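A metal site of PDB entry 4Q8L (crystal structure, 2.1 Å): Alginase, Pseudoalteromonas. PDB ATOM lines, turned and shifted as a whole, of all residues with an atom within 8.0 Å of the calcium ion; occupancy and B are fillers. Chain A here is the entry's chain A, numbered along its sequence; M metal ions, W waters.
The backbone carbonyl oxygen (O) of Thr 101 sits close to the backbone NH (N) of Val 110, 3.4 Å away.
N of Asp 108 lies within hydrogen-bond range of OD1 of Asp 117, at 2.9 Å.
The backbone carbonyl oxygen of Asp 100 lies within hydrogen-bond range of the backbone NH of Asn 112 (2.9 Å).
OD2 of Asp 100 sits at hydrogen-bond distance from N of Gly 114.
N of Gly 77 sits at hydrogen-bond distance from OD2 of Asp 100, 2.8 Å away.
N of Asp 100 sits at hydrogen-bond distance from O of Gly 78 (3.0 Å).
The nearest printed residue that does not touch the calcium ion is Thr 101 (4.4 Å).
The calcium ion is bound by O of Val 110, O of Ile 115, OD2 of Asp 108, OD1 of Asn 113, OD1 of Asp 100 and water W1.
The calcium ion has six donor atoms within binding distance.
Water W1 lies within hydrogen-bond range of O of Thr 101 (2.6 Å), OD2 of Asp 117 (2.6 Å) and N of Val 110 (3.3 Å).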
ATOM      1  N   ASP A  76      24.854   0.297 -33.102  1.00  0.00           N
ATOM      2  CA  ASP A  76      24.962   1.733 -32.898  1.00  0.00           C
ATOM      3  C   ASP A  76      23.882   2.155 -31.920  1.00  0.00           C
ATOM      4  O   ASP A  76      22.769   1.626 -31.969  1.00  0.00           O
ATOM      5  CB  ASP A  76      24.774   2.500 -34.213  1.00  0.00           C
ATOM      6  CG  ASP A  76      25.818   2.152 -35.261  1.00  0.00           C
ATOM      7  OD1 ASP A  76      25.556   2.419 -36.452  1.00  0.00           O
ATOM      8  OD2 ASP A  76      26.897   1.613 -34.919  1.00  0.00           O
ATOM      9  N   GLY A  77      24.209   3.090 -31.036  1.00  0.00           N
ATOM     10  CA  GLY A  77      23.268   3.544 -30.024  1.00  0.00           C
ATOM     11  C   GLY A  77      23.129   2.616 -28.821  1.00  0.00           C
ATOM     12  O   GLY A  77      22.437   2.946 -27.864  1.00  0.00           O
ATOM     13  N   GLY A  78      23.785   1.472 -28.863  1.00  0.00           N
ATOM     14  CA  GLY A  78      23.717   0.532 -27.753  1.00  0.00           C
ATOM     15  C   GLY A  78      24.484   0.977 -26.504  1.00  0.00           C
ATOM     16  O   GLY A  78      25.440   1.749 -26.579  1.00  0.00           O
ATOM     17  N   SER A  99      29.230   2.490 -24.303  1.00  0.00           N
ATOM     18  CA  SER A  99      27.993   3.083 -24.790  1.00  0.00           C
ATOM     19  C   SER A  99      28.154   4.127 -25.901  1.00  0.00           C
ATOM     20  O   SER A  99      29.168   4.814 -25.996  1.00  0.00           O
ATOM     21  CB  SER A  99      27.159   3.619 -23.618  1.00  0.00           C
ATOM     22  OG  SER A  99      27.451   4.959 -23.307  1.00  0.00           O
ATOM     23  N   ASP A 100      27.128   4.225 -26.736  1.00  0.00           N
ATOM     24  CA  ASP A 100      27.162   5.062 -27.929  1.00  0.00           C
ATOM     25  C   ASP A 100      26.034   6.083 -27.791  1.00  0.00           C
ATOM     26  O   ASP A 100      25.117   6.132 -28.615  1.00  0.00           O
ATOM     27  CB  ASP A 100      27.004   4.167 -29.173  1.00  0.00           C
ATOM     28  CG  ASP A 100      27.068   4.937 -30.490  1.00  0.00           C
ATOM     29  OD1 ASP A 100      27.504   6.091 -30.488  1.00  0.00           O
ATOM     30  OD2 ASP A 100      26.688   4.367 -31.535  1.00  0.00           O
ATOM     31  N   THR A 101      26.101   6.875 -26.721  1.00  0.00           N
ATOM     32  CA  THR A 101      25.063   7.840 -26.411  1.00  0.00           C
ATOM     33  C   THR A 101      25.613   9.260 -26.478  1.00  0.00           C
ATOM     34  O   THR A 101      26.781   9.481 -26.794  1.00  0.00           O
ATOM     35  CB  THR A 101      24.472   7.637 -24.999  1.00  0.00           C
ATOM     36  OG1 THR A 101      25.389   8.139 -24.006  1.00  0.00           O
ATOM     37  CG2 THR A 101      24.177   6.168 -24.720  1.00  0.00           C
ATOM     38  N   ASP A 102      24.755  10.226 -26.168  1.00  0.00           N
ATOM     39  CA  ASP A 102      25.199  11.615 -26.142  1.00  0.00           C
ATOM     40  C   ASP A 102      25.250  12.183 -24.726  1.00  0.00           C
ATOM     41  O   ASP A 102      25.209  13.396 -24.541  1.00  0.00           O
ATOM     42  CB  ASP A 102      24.349  12.501 -27.062  1.00  0.00           C
ATOM     43  CG  ASP A 102      22.896  12.538 -26.678  1.00  0.00           C
ATOM     44  OD1 ASP A 102      22.089  13.037 -27.483  1.00  0.00           O
ATOM     45  OD2 ASP A 102      22.558  12.083 -25.562  1.00  0.00           O
ATOM     46  N   ASN A 107      35.001  11.087 -24.220  1.00  0.00           N
ATOM     47  CA  ASN A 107      35.842  11.436 -25.349  1.00  0.00           C
ATOM     48  C   ASN A 107      35.034  11.649 -26.620  1.00  0.00           C
ATOM     49  O   ASN A 107      35.320  12.535 -27.425  1.00  0.00           O
ATOM     50  CB  ASN A 107      36.898  10.364 -25.584  1.00  0.00           C
ATOM     51  CG  ASN A 107      37.853  10.212 -24.403  1.00  0.00           C
ATOM     52  OD1 ASN A 107      37.815  11.006 -23.465  1.00  0.00           O
ATOM     53  ND2 ASN A 107      38.721   9.203 -24.459  1.00  0.00           N
ATOM     54  N   ASP A 108      34.015  10.815 -26.813  1.00  0.00           N
ATOM     55  CA  ASP A 108      33.166  10.953 -27.997  1.00  0.00           C
ATOM     56  C   ASP A 108      31.862  11.681 -27.650  1.00  0.00           C
ATOM     57  O   ASP A 108      31.638  12.810 -28.089  1.00  0.00           O
ATOM     58  CB  ASP A 108      32.916   9.591 -28.639  1.00  0.00           C
ATOM     59  CG  ASP A 108      32.001   9.684 -29.835  1.00  0.00           C
ATOM     60  OD1 ASP A 108      32.493   9.913 -30.968  1.00  0.00           O
ATOM     61  OD2 ASP A 108      30.776   9.536 -29.636  1.00  0.00           O
ATOM     62  N   SER A 109      31.032  11.034 -26.841  1.00  0.00           N
ATOM     63  CA  SER A 109      29.776  11.626 -26.381  1.00  0.00           C
ATOM     64  C   SER A 109      28.806  12.013 -27.501  1.00  0.00           C
ATOM     65  O   SER A 109      27.988  12.908 -27.341  1.00  0.00           O
ATOM     66  CB  SER A 109      30.044  12.823 -25.464  1.00  0.00           C
ATOM     67  OG  SER A 109      30.498  12.393 -24.186  1.00  0.00           O
ATOM     68  N   VAL A 110      28.901  11.322 -28.637  1.00  0.00           N
ATOM     69  CA  VAL A 110      28.005  11.566 -29.755  1.00  0.00           C
ATOM     70  C   VAL A 110      27.045  10.395 -29.909  1.00  0.00           C
ATOM     71  O   VAL A 110      27.477   9.264 -30.116  1.00  0.00           O
ATOM     72  CB  VAL A 110      28.804  11.752 -31.062  1.00  0.00           C
ATOM     73  CG1 VAL A 110      27.868  11.775 -32.286  1.00  0.00           C
ATOM     74  CG2 VAL A 110      29.656  13.028 -31.001  1.00  0.00           C
ATOM     75  N   ALA A 111      25.746  10.629 -29.790  1.00  0.00           N
ATOM     76  CA  ALA A 111      24.781   9.531 -29.911  1.00  0.00           C
ATOM     77  C   ALA A 111      24.848   8.814 -31.261  1.00  0.00           C
ATOM     78  O   ALA A 111      24.953   9.444 -32.314  1.00  0.00           O
ATOM     79  CB  ALA A 111      23.357  10.026 -29.662  1.00  0.00           C
ATOM     80  N   ASN A 112      24.800   7.492 -31.213  1.00  0.00           N
ATOM     81  CA  ASN A 112      24.450   6.698 -32.384  1.00  0.00           C
ATOM     82  C   ASN A 112      25.382   6.884 -33.571  1.00  0.00           C
ATOM     83  O   ASN A 112      24.917   6.883 -34.711  1.00  0.00           O
ATOM     84  CB  ASN A 112      23.001   7.044 -32.796  1.00  0.00           C
ATOM     85  CG  ASN A 112      22.411   6.029 -33.769  1.00  0.00           C
ATOM     86  OD1 ASN A 112      22.662   4.826 -33.669  1.00  0.00           O
ATOM     87  ND2 ASN A 112      21.603   6.521 -34.719  1.00  0.00           N
ATOM     88  N   ASN A 113      26.681   7.027 -33.322  1.00  0.00           N
ATOM     89  CA  ASN A 113      27.631   7.137 -34.415  1.00  0.00           C
ATOM     90  C   ASN A 113      28.587   5.947 -34.481  1.00  0.00           C
ATOM     91  O   ASN A 113      29.556   5.969 -35.220  1.00  0.00           O
ATOM     92  CB  ASN A 113      28.431   8.455 -34.350  1.00  0.00           C
ATOM     93  CG  ASN A 113      29.432   8.469 -33.212  1.00  0.00           C
ATOM     94  OD1 ASN A 113      29.351   7.622 -32.326  1.00  0.00           O
ATOM     95  ND2 ASN A 113      30.380   9.417 -33.215  1.00  0.00           N
ATOM     96  N   GLY A 114      28.310   4.899 -33.704  1.00  0.00           N
ATOM     97  CA  GLY A 114      29.149   3.704 -33.730  1.00  0.00           C
ATOM     98  C   GLY A 114      30.498   3.844 -33.041  1.00  0.00           C
ATOM     99  O   GLY A 114      31.346   2.943 -33.089  1.00  0.00           O
ATOM    100  N   ILE A 115      30.716   4.982 -32.403  1.00  0.00           N
ATOM    101  CA  ILE A 115      31.929   5.178 -31.614  1.00  0.00           C
ATOM    102  C   ILE A 115      31.529   5.054 -30.155  1.00  0.00           C
ATOM    103  O   ILE A 115      30.815   5.897 -29.635  1.00  0.00           O
ATOM    104  CB  ILE A 115      32.566   6.547 -31.869  1.00  0.00           C
ATOM    105  CG1 ILE A 115      32.977   6.663 -33.346  1.00  0.00           C
ATOM    106  CG2 ILE A 115      33.792   6.758 -30.955  1.00  0.00           C
ATOM    107  CD1 ILE A 115      33.857   7.851 -33.645  1.00  0.00           C
ATOM    108  N   PHE A 116      31.970   3.993 -29.489  1.00  0.00           N
ATOM    109  CA  PHE A 116      31.508   3.744 -28.136  1.00  0.00           C
ATOM    110  C   PHE A 116      32.426   4.366 -27.105  1.00  0.00           C
ATOM    111  O   PHE A 116      33.625   4.163 -27.152  1.00  0.00           O
ATOM    112  CB  PHE A 116      31.368   2.240 -27.900  1.00  0.00           C
ATOM    113  CG  PHE A 116      30.327   1.596 -28.761  1.00  0.00           C
ATOM    114  CD1 PHE A 116      30.650   1.111 -30.021  1.00  0.00           C
ATOM    115  CD2 PHE A 116      29.016   1.514 -28.329  1.00  0.00           C
ATOM    116  CE1 PHE A 116      29.687   0.549 -30.825  1.00  0.00           C
ATOM    117  CE2 PHE A 116      28.043   0.925 -29.125  1.00  0.00           C
ATOM    118  CZ  PHE A 116      28.382   0.450 -30.381  1.00  0.00           C
ATOM    119  N   ASP A 117      31.847   5.123 -26.179  1.00  0.00           N
ATOM    120  CA  ASP A 117      32.601   5.573 -25.020  1.00  0.00           C
ATOM    121  C   ASP A 117      32.734   4.415 -24.055  1.00  0.00           C
ATOM    122  O   ASP A 117      31.770   3.676 -23.819  1.00  0.00           O
ATOM    123  CB  ASP A 117      31.893   6.741 -24.329  1.00  0.00           C
ATOM    124  CG  ASP A 117      31.807   7.978 -25.203  1.00  0.00           C
ATOM    125  OD1 ASP A 117      32.888   8.504 -25.562  1.00  0.00           O
ATOM    126  OD2 ASP A 117      30.682   8.415 -25.510  1.00  0.00           O
ATOM    127  N   THR A 136      37.687   5.032 -26.080  1.00  0.00           N
ATOM    128  CA  THR A 136      36.648   4.786 -27.063  1.00  0.00           C
ATOM    129  C   THR A 136      36.993   3.553 -27.900  1.00  0.00           C
ATOM    130  O   THR A 136      38.152   3.153 -27.981  1.00  0.00           O
ATOM    131  CB  THR A 136      36.464   5.961 -28.050  1.00  0.00           C
ATOM    132  OG1 THR A 136      37.704   6.231 -28.703  1.00  0.00           O
ATOM    133  CG2 THR A 136      35.982   7.219 -27.330  1.00  0.00           C
ATOM    134  N   MET A 137      35.968   2.952 -28.501  1.00  0.00           N
ATOM    135  CA  MET A 137      36.162   1.806 -29.369  1.00  0.00           C
ATOM    136  C   MET A 137      35.036   1.737 -30.379  1.00  0.00           C
ATOM    137  O   MET A 137      33.998   2.392 -30.210  1.00  0.00           O
ATOM    138  CB  MET A 137      36.181   0.508 -28.551  1.00  0.00           C
ATOM    139  CG  MET A 137      34.832   0.156 -27.928  1.00  0.00           C
ATOM    140  SD  MET A 137      34.943  -1.241 -26.778  1.00  0.00           S
ATOM    141  CE  MET A 137      35.469  -2.561 -27.878  1.00  0.00           C
HETATM  142 CA    CA M   1      29.243   7.696 -29.911  1.00  0.00          CA
HETATM  143  O   HOH W   1      28.918   8.217 -27.389  1.00  0.00           O
